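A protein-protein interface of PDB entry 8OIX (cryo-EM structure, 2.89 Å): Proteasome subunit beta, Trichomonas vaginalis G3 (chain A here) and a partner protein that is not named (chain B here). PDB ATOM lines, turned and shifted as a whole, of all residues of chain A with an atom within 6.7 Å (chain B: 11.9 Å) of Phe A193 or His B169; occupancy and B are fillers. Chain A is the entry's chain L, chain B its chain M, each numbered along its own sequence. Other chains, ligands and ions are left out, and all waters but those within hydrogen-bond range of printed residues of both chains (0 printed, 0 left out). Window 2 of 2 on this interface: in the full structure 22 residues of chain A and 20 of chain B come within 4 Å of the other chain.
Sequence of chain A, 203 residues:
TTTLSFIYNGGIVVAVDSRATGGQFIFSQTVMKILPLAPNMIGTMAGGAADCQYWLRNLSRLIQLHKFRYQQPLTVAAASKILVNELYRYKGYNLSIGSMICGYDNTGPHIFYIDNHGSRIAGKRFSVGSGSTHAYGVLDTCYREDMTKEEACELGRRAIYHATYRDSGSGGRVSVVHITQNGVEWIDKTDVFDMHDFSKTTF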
ATOM      1  N   TYR A 161     -12.690 -19.251 -14.287  1.00  0.00           N
ATOM      2  CA  TYR A 161     -12.750 -17.821 -14.571  1.00  0.00           C
ATOM      3  C   TYR A 161     -12.197 -17.001 -13.412  1.00  0.00           C
ATOM      4  O   TYR A 161     -11.439 -16.047 -13.623  1.00  0.00           O
ATOM      5  CB  TYR A 161     -14.187 -17.403 -14.877  1.00  0.00           C
ATOM      6  CG  TYR A 161     -14.488 -15.971 -14.498  1.00  0.00           C
ATOM      7  CD1 TYR A 161     -13.921 -14.914 -15.196  1.00  0.00           C
ATOM      8  CD2 TYR A 161     -15.329 -15.679 -13.435  1.00  0.00           C
ATOM      9  CE1 TYR A 161     -14.186 -13.607 -14.847  1.00  0.00           C
ATOM     10  CE2 TYR A 161     -15.601 -14.375 -13.080  1.00  0.00           C
ATOM     11  CZ  TYR A 161     -15.028 -13.343 -13.789  1.00  0.00           C
ATOM     12  OH  TYR A 161     -15.297 -12.041 -13.441  1.00  0.00           O
ATOM     13  N   THR A 164      -8.492 -17.337 -13.380  1.00  0.00           N
ATOM     14  CA  THR A 164      -7.883 -16.507 -14.413  1.00  0.00           C
ATOM     15  C   THR A 164      -7.868 -15.047 -13.997  1.00  0.00           C
ATOM     16  O   THR A 164      -6.893 -14.329 -14.246  1.00  0.00           O
ATOM     17  CB  THR A 164      -8.620 -16.672 -15.742  1.00  0.00           C
ATOM     18  OG1 THR A 164      -9.980 -16.247 -15.594  1.00  0.00           O
ATOM     19  CG2 THR A 164      -8.573 -18.114 -16.214  1.00  0.00           C
ATOM     20  N   GLY A 172      -7.265 -16.944 -20.887  1.00  0.00           N
ATOM     21  CA  GLY A 172      -7.664 -17.520 -22.159  1.00  0.00           C
ATOM     22  C   GLY A 172      -9.119 -17.931 -22.143  1.00  0.00           C
ATOM     23  O   GLY A 172      -9.992 -17.124 -21.846  1.00  0.00           O
ATOM     24  N   THR A 190     -15.192 -21.437 -23.381  1.00  0.00           N
ATOM     25  CA  THR A 190     -15.824 -20.165 -23.056  1.00  0.00           C
ATOM     26  C   THR A 190     -14.747 -19.141 -22.726  1.00  0.00           C
ATOM     27  O   THR A 190     -13.979 -19.332 -21.783  1.00  0.00           O
ATOM     28  CB  THR A 190     -16.796 -20.314 -21.889  1.00  0.00           C
ATOM     29  OG1 THR A 190     -17.800 -21.280 -22.224  1.00  0.00           O
ATOM     30  CG2 THR A 190     -17.470 -18.990 -21.599  1.00  0.00           C
ATOM     31  N   ASP A 191     -14.696 -18.062 -23.498  1.00  0.00           N
ATOM     32  CA  ASP A 191     -13.762 -16.978 -23.219  1.00  0.00           C
ATOM     33  C   ASP A 191     -14.067 -16.352 -21.864  1.00  0.00           C
ATOM     34  O   ASP A 191     -15.179 -15.869 -21.631  1.00  0.00           O
ATOM     35  CB  ASP A 191     -13.842 -15.931 -24.329  1.00  0.00           C
ATOM     36  CG  ASP A 191     -12.817 -14.825 -24.171  1.00  0.00           C
ATOM     37  OD1 ASP A 191     -11.968 -14.912 -23.259  1.00  0.00           O
ATOM     38  OD2 ASP A 191     -12.860 -13.862 -24.963  1.00  0.00           O
ATOM     39  N   VAL A 192     -13.077 -16.371 -20.965  1.00  0.00           N
ATOM     40  CA  VAL A 192     -13.249 -15.781 -19.641  1.00  0.00           C
ATOM     41  C   VAL A 192     -13.520 -14.288 -19.733  1.00  0.00           C
ATOM     42  O   VAL A 192     -14.053 -13.696 -18.790  1.00  0.00           O
ATOM     43  CB  VAL A 192     -12.013 -16.035 -18.754  1.00  0.00           C
ATOM     44  CG1 VAL A 192     -11.780 -17.513 -18.569  1.00  0.00           C
ATOM     45  CG2 VAL A 192     -10.787 -15.365 -19.337  1.00  0.00           C
ATOM     46  N   PHE A 193     -13.149 -13.660 -20.850  1.00  0.00           N
ATOM     47  CA  PHE A 193     -13.475 -12.256 -21.058  1.00  0.00           C
ATOM     48  C   PHE A 193     -14.983 -12.055 -21.100  1.00  0.00           C
ATOM     49  O   PHE A 193     -15.502 -11.050 -20.600  1.00  0.00           O
ATOM     50  CB  PHE A 193     -12.825 -11.768 -22.353  1.00  0.00           C
ATOM     51  CG  PHE A 193     -12.841 -10.281 -22.525  1.00  0.00           C
ATOM     52  CD1 PHE A 193     -12.949  -9.440 -21.433  1.00  0.00           C
ATOM     53  CD2 PHE A 193     -12.743  -9.722 -23.785  1.00  0.00           C
ATOM     54  CE1 PHE A 193     -12.960  -8.072 -21.598  1.00  0.00           C
ATOM     55  CE2 PHE A 193     -12.756  -8.357 -23.955  1.00  0.00           C
ATOM     56  CZ  PHE A 193     -12.862  -7.530 -22.862  1.00  0.00           C
ATOM     57  N   ASP A 194     -15.705 -13.005 -21.696  1.00  0.00           N
ATOM     58  CA  ASP A 194     -17.160 -12.947 -21.716  1.00  0.00           C
ATOM     59  C   ASP A 194     -17.762 -13.326 -20.370  1.00  0.00           C
ATOM     60  O   ASP A 194     -18.844 -12.842 -20.021  1.00  0.00           O
ATOM     61  CB  ASP A 194     -17.704 -13.865 -22.810  1.00  0.00           C
ATOM     62  CG  ASP A 194     -17.025 -13.643 -24.146  1.00  0.00           C
ATOM     63  OD1 ASP A 194     -16.457 -12.550 -24.352  1.00  0.00           O
ATOM     64  OD2 ASP A 194     -17.057 -14.563 -24.990  1.00  0.00           O
ATOM     65  N   MET A 195     -17.083 -14.187 -19.608  1.00  0.00           N
ATOM     66  CA  MET A 195     -17.606 -14.607 -18.313  1.00  0.00           C
ATOM     67  C   MET A 195     -17.551 -13.487 -17.286  1.00  0.00           C
ATOM     68  O   MET A 195     -18.380 -13.452 -16.370  1.00  0.00           O
ATOM     69  CB  MET A 195     -16.828 -15.815 -17.796  1.00  0.00           C
ATOM     70  CG  MET A 195     -16.790 -16.984 -18.751  1.00  0.00           C
ATOM     71  SD  MET A 195     -15.999 -18.414 -18.003  1.00  0.00           S
ATOM     72  CE  MET A 195     -17.094 -18.681 -16.614  1.00  0.00           C
ATOM     73  N   HIS A 196     -16.585 -12.580 -17.409  1.00  0.00           N
ATOM     74  CA  HIS A 196     -16.460 -11.489 -16.453  1.00  0.00           C
ATOM     75  C   HIS A 196     -17.698 -10.604 -16.488  1.00  0.00           C
ATOM     76  O   HIS A 196     -18.172 -10.218 -17.561  1.00  0.00           O
ATOM     77  CB  HIS A 196     -15.209 -10.664 -16.753  1.00  0.00           C
ATOM     78  CG  HIS A 196     -14.910  -9.625 -15.718  1.00  0.00           C
ATOM     79  ND1 HIS A 196     -14.149  -9.886 -14.601  1.00  0.00           N
ATOM     80  CD2 HIS A 196     -15.279  -8.325 -15.626  1.00  0.00           C
ATOM     81  CE1 HIS A 196     -14.057  -8.792 -13.868  1.00  0.00           C
ATOM     82  NE2 HIS A 196     -14.733  -7.830 -14.468  1.00  0.00           N
ATOM     83  N   ASP A 197     -18.220 -10.283 -15.309  1.00  0.00           N
ATOM     84  CA  ASP A 197     -19.386  -9.419 -15.174  1.00  0.00           C
ATOM     85  C   ASP A 197     -18.881  -8.003 -14.929  1.00  0.00           C
ATOM     86  O   ASP A 197     -18.399  -7.689 -13.837  1.00  0.00           O
ATOM     87  CB  ASP A 197     -20.289  -9.895 -14.038  1.00  0.00           C
ATOM     88  CG  ASP A 197     -21.666  -9.256 -14.074  1.00  0.00           C
ATOM     89  OD1 ASP A 197     -21.787  -8.102 -14.532  1.00  0.00           O
ATOM     90  OD2 ASP A 197     -22.634  -9.916 -13.643  1.00  0.00           O
ATOM     91  N   PHE A 198     -18.991  -7.154 -15.945  1.00  0.00           N
ATOM     92  CA  PHE A 198     -18.499  -5.788 -15.865  1.00  0.00           C
ATOM     93  C   PHE A 198     -19.505  -4.829 -15.247  1.00  0.00           C
ATOM     94  O   PHE A 198     -19.197  -3.643 -15.099  1.00  0.00           O
ATOM     95  CB  PHE A 198     -18.085  -5.301 -17.254  1.00  0.00           C
ATOM     96  CG  PHE A 198     -16.893  -6.022 -17.806  1.00  0.00           C
ATOM     97  CD1 PHE A 198     -17.044  -7.207 -18.502  1.00  0.00           C
ATOM     98  CD2 PHE A 198     -15.618  -5.530 -17.602  1.00  0.00           C
ATOM     99  CE1 PHE A 198     -15.946  -7.877 -19.000  1.00  0.00           C
ATOM    100  CE2 PHE A 198     -14.518  -6.197 -18.095  1.00  0.00           C
ATOM    101  CZ  PHE A 198     -14.682  -7.371 -18.795  1.00  0.00           C
ATOM    102  N   LEU B 144      -1.885 -23.302 -33.962  1.00  0.00           N
ATOM    103  CA  LEU B 144      -2.117 -21.876 -33.830  1.00  0.00           C
ATOM    104  C   LEU B 144      -2.540 -21.280 -35.162  1.00  0.00           C
ATOM    105  O   LEU B 144      -2.125 -21.740 -36.229  1.00  0.00           O
ATOM    106  CB  LEU B 144      -0.860 -21.167 -33.325  1.00  0.00           C
ATOM    107  CG  LEU B 144      -0.550 -21.428 -31.857  1.00  0.00           C
ATOM    108  CD1 LEU B 144       0.836 -20.947 -31.504  1.00  0.00           C
ATOM    109  CD2 LEU B 144      -1.590 -20.721 -31.015  1.00  0.00           C
ATOM    110  N   HIS B 145      -3.380 -20.250 -35.088  1.00  0.00           N
ATOM    111  CA  HIS B 145      -3.652 -19.440 -36.266  1.00  0.00           C
ATOM    112  C   HIS B 145      -2.496 -18.499 -36.557  1.00  0.00           C
ATOM    113  O   HIS B 145      -2.214 -18.203 -37.723  1.00  0.00           O
ATOM    114  CB  HIS B 145      -4.945 -18.652 -36.074  1.00  0.00           C
ATOM    115  CG  HIS B 145      -6.165 -19.509 -35.967  1.00  0.00           C
ATOM    116  ND1 HIS B 145      -7.115 -19.333 -34.986  1.00  0.00           N
ATOM    117  CD2 HIS B 145      -6.590 -20.551 -36.720  1.00  0.00           C
ATOM    118  CE1 HIS B 145      -8.074 -20.229 -35.138  1.00  0.00           C
ATOM    119  NE2 HIS B 145      -7.780 -20.980 -36.182  1.00  0.00           N
ATOM    120  N   TYR B 146      -1.829 -18.017 -35.513  1.00  0.00           N
ATOM    121  CA  TYR B 146      -0.636 -17.202 -35.658  1.00  0.00           C
ATOM    122  C   TYR B 146       0.245 -17.418 -34.439  1.00  0.00           C
ATOM    123  O   TYR B 146      -0.218 -17.843 -33.378  1.00  0.00           O
ATOM    124  CB  TYR B 146      -0.977 -15.717 -35.824  1.00  0.00           C
ATOM    125  CG  TYR B 146      -1.681 -15.112 -34.632  1.00  0.00           C
ATOM    126  CD1 TYR B 146      -0.968 -14.653 -33.534  1.00  0.00           C
ATOM    127  CD2 TYR B 146      -3.061 -14.995 -34.608  1.00  0.00           C
ATOM    128  CE1 TYR B 146      -1.607 -14.101 -32.450  1.00  0.00           C
ATOM    129  CE2 TYR B 146      -3.708 -14.443 -33.530  1.00  0.00           C
ATOM    130  CZ  TYR B 146      -2.977 -13.998 -32.452  1.00  0.00           C
ATOM    131  OH  TYR B 146      -3.621 -13.446 -31.373  1.00  0.00           O
ATOM    132  N   ALA B 157       3.916 -10.224 -31.004  1.00  0.00           N
ATOM    133  CA  ALA B 157       2.658 -10.863 -30.625  1.00  0.00           C
ATOM    134  C   ALA B 157       1.495  -9.884 -30.524  1.00  0.00           C
ATOM    135  O   ALA B 157       0.413 -10.197 -31.049  1.00  0.00           O
ATOM    136  CB  ALA B 157       2.854 -11.654 -29.329  1.00  0.00           C
ATOM    137  N   PRO B 158       1.619  -8.720 -29.874  1.00  0.00           N
ATOM    138  CA  PRO B 158       0.516  -7.746 -29.922  1.00  0.00           C
ATOM    139  C   PRO B 158       0.156  -7.303 -31.324  1.00  0.00           C
ATOM    140  O   PRO B 158      -1.014  -7.002 -31.579  1.00  0.00           O
ATOM    141  CB  PRO B 158       1.045  -6.573 -29.088  1.00  0.00           C
ATOM    142  CG  PRO B 158       2.016  -7.174 -28.186  1.00  0.00           C
ATOM    143  CD  PRO B 158       2.659  -8.297 -28.923  1.00  0.00           C
ATOM    144  N   LEU B 160       0.086  -9.155 -34.029  1.00  0.00           N
ATOM    145  CA  LEU B 160      -0.810 -10.174 -34.560  1.00  0.00           C
ATOM    146  C   LEU B 160      -2.134 -10.187 -33.805  1.00  0.00           C
ATOM    147  O   LEU B 160      -3.196 -10.388 -34.408  1.00  0.00           O
ATOM    148  CB  LEU B 160      -0.132 -11.536 -34.493  1.00  0.00           C
ATOM    149  CG  LEU B 160       1.248 -11.600 -35.143  1.00  0.00           C
ATOM    150  CD1 LEU B 160       1.971 -12.876 -34.749  1.00  0.00           C
ATOM    151  CD2 LEU B 160       1.121 -11.492 -36.650  1.00  0.00           C
ATOM    152  N   ASP B 161      -2.092  -9.973 -32.489  1.00  0.00           N
ATOM    153  CA  ASP B 161      -3.327  -9.903 -31.716  1.00  0.00           C
ATOM    154  C   ASP B 161      -4.224  -8.782 -32.217  1.00  0.00           C
ATOM    155  O   ASP B 161      -5.438  -8.957 -32.342  1.00  0.00           O
ATOM    156  CB  ASP B 161      -3.015  -9.705 -30.234  1.00  0.00           C
ATOM    157  CG  ASP B 161      -2.175 -10.820 -29.665  1.00  0.00           C
ATOM    158  OD1 ASP B 161      -1.925 -11.805 -30.389  1.00  0.00           O
ATOM    159  OD2 ASP B 161      -1.772 -10.717 -28.492  1.00  0.00           O
ATOM    160  N   SER B 162      -3.642  -7.619 -32.507  1.00  0.00           N
ATOM    161  CA  SER B 162      -4.427  -6.525 -33.061  1.00  0.00           C
ATOM    162  C   SER B 162      -4.927  -6.864 -34.457  1.00  0.00           C
ATOM    163  O   SER B 162      -6.098  -6.628 -34.773  1.00  0.00           O
ATOM    164  CB  SER B 162      -3.598  -5.245 -33.080  1.00  0.00           C
ATOM    165  OG  SER B 162      -3.120  -4.945 -31.783  1.00  0.00           O
ATOM    166  N   ALA B 163      -4.060  -7.434 -35.298  1.00  0.00           N
ATOM    167  CA  ALA B 163      -4.465  -7.767 -36.658  1.00  0.00           C
ATOM    168  C   ALA B 163      -5.626  -8.754 -36.683  1.00  0.00           C
ATOM    169  O   ALA B 163      -6.458  -8.704 -37.595  1.00  0.00           O
ATOM    170  CB  ALA B 163      -3.275  -8.329 -37.435  1.00  0.00           C
ATOM    171  N   PHE B 164      -5.703  -9.654 -35.701  1.00  0.00           N
ATOM    172  CA  PHE B 164      -6.718 -10.698 -35.714  1.00  0.00           C
ATOM    173  C   PHE B 164      -7.680 -10.678 -34.535  1.00  0.00           C
ATOM    174  O   PHE B 164      -8.798 -11.186 -34.674  1.00  0.00           O
ATOM    175  CB  PHE B 164      -6.054 -12.080 -35.790  1.00  0.00           C
ATOM    176  CG  PHE B 164      -5.046 -12.200 -36.892  1.00  0.00           C
ATOM    177  CD1 PHE B 164      -5.446 -12.170 -38.215  1.00  0.00           C
ATOM    178  CD2 PHE B 164      -3.701 -12.343 -36.610  1.00  0.00           C
ATOM    179  CE1 PHE B 164      -4.522 -12.277 -39.231  1.00  0.00           C
ATOM    180  CE2 PHE B 164      -2.775 -12.450 -37.623  1.00  0.00           C
ATOM    181  CZ  PHE B 164      -3.189 -12.416 -38.935  1.00  0.00           C
ATOM    182  N   GLY B 165      -7.295 -10.116 -33.392  1.00  0.00           N
ATOM    183  CA  GLY B 165      -8.178 -10.117 -32.242  1.00  0.00           C
ATOM    184  C   GLY B 165      -8.359 -11.457 -31.572  1.00  0.00           C
ATOM    185  O   GLY B 165      -9.252 -11.595 -30.731  1.00  0.00           O
ATOM    186  N   THR B 166      -7.542 -12.454 -31.921  1.00  0.00           N
ATOM    187  CA  THR B 166      -7.727 -13.791 -31.368  1.00  0.00           C
ATOM    188  C   THR B 166      -7.426 -13.825 -29.875  1.00  0.00           C
ATOM    189  O   THR B 166      -8.122 -14.502 -29.112  1.00  0.00           O
ATOM    190  CB  THR B 166      -6.851 -14.792 -32.118  1.00  0.00           C
ATOM    191  OG1 THR B 166      -7.154 -14.734 -33.517  1.00  0.00           O
ATOM    192  CG2 THR B 166      -7.097 -16.208 -31.612  1.00  0.00           C
ATOM    193  N   ILE B 167      -6.395 -13.102 -29.435  1.00  0.00           N
ATOM    194  CA  ILE B 167      -6.097 -13.047 -28.008  1.00  0.00           C
ATOM    195  C   ILE B 167      -7.166 -12.250 -27.273  1.00  0.00           C
ATOM    196  O   ILE B 167      -7.577 -12.611 -26.165  1.00  0.00           O
ATOM    197  CB  ILE B 167      -4.689 -12.470 -27.779  1.00  0.00           C
ATOM    198  CG1 ILE B 167      -3.626 -13.472 -28.228  1.00  0.00           C
ATOM    199  CG2 ILE B 167      -4.482 -12.120 -26.317  1.00  0.00           C
ATOM    200  CD1 ILE B 167      -3.481 -14.668 -27.333  1.00  0.00           C
ATOM    201  N   HIS B 168      -7.638 -11.159 -27.883  1.00  0.00           N
ATOM    202  CA  HIS B 168      -8.666 -10.333 -27.257  1.00  0.00           C
ATOM    203  C   HIS B 168      -9.948 -11.124 -27.042  1.00  0.00           C
ATOM    204  O   HIS B 168     -10.564 -11.059 -25.972  1.00  0.00           O
ATOM    205  CB  HIS B 168      -8.930  -9.100 -28.123  1.00  0.00           C
ATOM    206  CG  HIS B 168      -9.799  -8.071 -27.471  1.00  0.00           C
ATOM    207  ND1 HIS B 168      -9.686  -7.738 -26.139  1.00  0.00           N
ATOM    208  CD2 HIS B 168     -10.789  -7.296 -27.969  1.00  0.00           C
ATOM    209  CE1 HIS B 168     -10.570  -6.802 -25.844  1.00  0.00           C
ATOM    210  NE2 HIS B 168     -11.254  -6.517 -26.937  1.00  0.00           N
ATOM    211  N   HIS B 169     -10.365 -11.882 -28.053  1.00  0.00           N
ATOM    212  CA  HIS B 169     -11.555 -12.727 -27.979  1.00  0.00           C
ATOM    213  C   HIS B 169     -11.169 -14.104 -28.508  1.00  0.00           C
ATOM    214  O   HIS B 169     -11.080 -14.310 -29.722  1.00  0.00           O
ATOM    215  CB  HIS B 169     -12.708 -12.119 -28.767  1.00  0.00           C
ATOM    216  CG  HIS B 169     -13.289 -10.895 -28.132  1.00  0.00           C
ATOM    217  ND1 HIS B 169     -13.460  -9.711 -28.814  1.00  0.00           N
ATOM    218  CD2 HIS B 169     -13.740 -10.673 -26.875  1.00  0.00           C
ATOM    219  CE1 HIS B 169     -13.990  -8.811 -28.005  1.00  0.00           C
ATOM    220  NE2 HIS B 169     -14.170  -9.370 -26.822  1.00  0.00           N
ATOM    221  N   ASN B 170     -10.937 -15.043 -27.588  1.00  0.00           N
ATOM    222  CA  ASN B 170     -10.382 -16.339 -27.963  1.00  0.00           C
ATOM    223  C   ASN B 170     -11.368 -17.163 -28.780  1.00  0.00           C
ATOM    224  O   ASN B 170     -10.980 -17.817 -29.754  1.00  0.00           O
ATOM    225  CB  ASN B 170      -9.961 -17.105 -26.710  1.00  0.00           C
ATOM    226  CG  ASN B 170      -9.300 -16.217 -25.682  1.00  0.00           C
ATOM    227  OD1 ASN B 170      -9.752 -16.128 -24.543  1.00  0.00           O
ATOM    228  ND2 ASN B 170      -8.222 -15.552 -26.077  1.00  0.00           N
ATOM    229  N   THR B 171     -12.643 -17.145 -28.402  1.00  0.00           N
ATOM    230  CA  THR B 171     -13.618 -18.071 -28.957  1.00  0.00           C
ATOM    231  C   THR B 171     -14.226 -17.606 -30.272  1.00  0.00           C
ATOM    232  O   THR B 171     -14.904 -18.400 -30.932  1.00  0.00           O
ATOM    233  CB  THR B 171     -14.737 -18.311 -27.944  1.00  0.00           C
ATOM    234  OG1 THR B 171     -15.434 -17.083 -27.704  1.00  0.00           O
ATOM    235  CG2 THR B 171     -14.141 -18.793 -26.642  1.00  0.00           C
ATOM    236  N   ARG B 172     -14.011 -16.357 -30.671  1.00  0.00           N
ATOM    237  CA  ARG B 172     -14.548 -15.899 -31.938  1.00  0.00           C
ATOM    238  C   ARG B 172     -13.795 -16.554 -33.095  1.00  0.00           C
ATOM    239  O   ARG B 172     -12.623 -16.913 -32.959  1.00  0.00           O
ATOM    240  CB  ARG B 172     -14.461 -14.379 -32.043  1.00  0.00           C
ATOM    241  CG  ARG B 172     -15.229 -13.652 -30.955  1.00  0.00           C
ATOM    242  CD  ARG B 172     -15.296 -12.161 -31.221  1.00  0.00           C
ATOM    243  NE  ARG B 172     -16.031 -11.459 -30.176  1.00  0.00           N
ATOM    244  CZ  ARG B 172     -16.257 -10.153 -30.167  1.00  0.00           C
ATOM    245  NH1 ARG B 172     -15.824  -9.370 -31.142  1.00  0.00           N
ATOM    246  NH2 ARG B 172     -16.933  -9.618 -29.154  1.00  0.00           N
ATOM    247  N   PRO B 173     -14.454 -16.740 -34.239  1.00  0.00           N
ATOM    248  CA  PRO B 173     -13.764 -17.327 -35.394  1.00  0.00           C
ATOM    249  C   PRO B 173     -12.600 -16.459 -35.849  1.00  0.00           C
ATOM    250  O   PRO B 173     -12.675 -15.229 -35.843  1.00  0.00           O
ATOM    251  CB  PRO B 173     -14.863 -17.410 -36.459  1.00  0.00           C
ATOM    252  CG  PRO B 173     -15.877 -16.402 -36.044  1.00  0.00           C
ATOM    253  CD  PRO B 173     -15.851 -16.393 -34.548  1.00  0.00           C
ATOM    254  N   PHE B 174     -11.520 -17.118 -36.241  1.00  0.00           N
ATOM    255  CA  PHE B 174     -10.343 -16.409 -36.723  1.00  0.00           C
ATOM    256  C   PHE B 174     -10.669 -15.713 -38.039  1.00  0.00           C
ATOM    257  O   PHE B 174     -11.196 -16.353 -38.958  1.00  0.00           O
ATOM    258  CB  PHE B 174      -9.184 -17.386 -36.898  1.00  0.00           C
ATOM    259  CG  PHE B 174      -7.902 -16.741 -37.329  1.00  0.00           C
ATOM    260  CD1 PHE B 174      -7.152 -16.000 -36.434  1.00  0.00           C
ATOM    261  CD2 PHE B 174      -7.435 -16.895 -38.621  1.00  0.00           C
ATOM    262  CE1 PHE B 174      -5.967 -15.414 -36.826  1.00  0.00           C
ATOM    263  CE2 PHE B 174      -6.252 -16.310 -39.017  1.00  0.00           C
ATOM    264  CZ  PHE B 174      -5.517 -15.570 -38.118  1.00  0.00           C
ATOM    265  N   PRO B 175     -10.391 -14.415 -38.167  1.00  0.00           N
ATOM    266  CA  PRO B 175     -10.812 -13.682 -39.368  1.00  0.00           C
ATOM    267  C   PRO B 175     -10.212 -14.269 -40.636  1.00  0.00           C
ATOM    268  O   PRO B 175      -9.064 -14.714 -40.658  1.00  0.00           O
ATOM    269  CB  PRO B 175     -10.305 -12.258 -39.110  1.00  0.00           C
ATOM    270  CG  PRO B 175      -9.237 -12.406 -38.074  1.00  0.00           C
ATOM    271  CD  PRO B 175      -9.664 -13.555 -37.219  1.00  0.00           C
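The backbone carbonyl oxygen of Gly A172 sits close to the side-chain amide oxygen of Asn B170, at 2.9 Å. The side-chain amide oxygen (OD1) of Asn B170 sits close to the side-chain carboxylate (OD1) of Asp A191 (2.8 Å).
A ring nitrogen (ND1) of His B169 sits close to the guanidinium group (NH1) of Arg B172. O of Gly A172 lies close to N of Val A192 (3.3 Å). The backbone carbonyl oxygen (O) of Ile B167 sits at hydrogen-bond distance from the side-chain amide nitrogen (ND2) of Asn B170 (3.0 Å). ND2 of Asn B170 sits close to O of Thr B166 (3.2 Å). The side-chain carboxylate (OD1) of Asp A191 sits at hydrogen-bond distance from the backbone NH (N) of Phe A193 (3.0 Å).
Of the 12 printed residues of chain A, 4 touch a printed residue of chain B. Hydrophobic or aromatic side chains of chain A within 4 Å of the printed part of chain B: Phe A193. Hydrophobic or aromatic side chains of chain B that line the printed part of chain A: His B168 and His B169. Among the printed residues, no Asp or Glu carboxylate lies within 4 Å of a Lys or Arg side-chain nitrogen of the other chain.
Among the printed residues, merely in contact across the chains: Thr A190 with Thr B171, Asp A191 with His B168, Asp A191 with His B169, Asp A191 with Thr B171, Phe A193 with His B168 and Phe A193 with His B169.
His B169 touches just these residues of chain A: Asp A191 and Phe A193. Asp A191 touches four residues of chain B. No residue of chain B comes within 4 Å of Val A192. No residue of chain B comes within 4 Å of Asp A194. Of the printed residues of chain A, His B168 touches Asp A191 and Phe A193. Printed residues of chain A within 4 Å of Thr B171: Thr A190 (3.98 Å) and Asp A191 (3.3 Å). Printed residues of chain B within 4 Å of Thr A190: Thr B171 (3.98 Å). Of the printed residues of chain A, Asn B170 touches Gly A172 (2.9 Å) and Asp A191 (2.8 Å). The nearest residue of chain B that does not touch Phe A193 is Asn B170 (5.6 Å). The nearest residue of chain A that does not touch His B169 is Asp A194 (4.2 Å).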
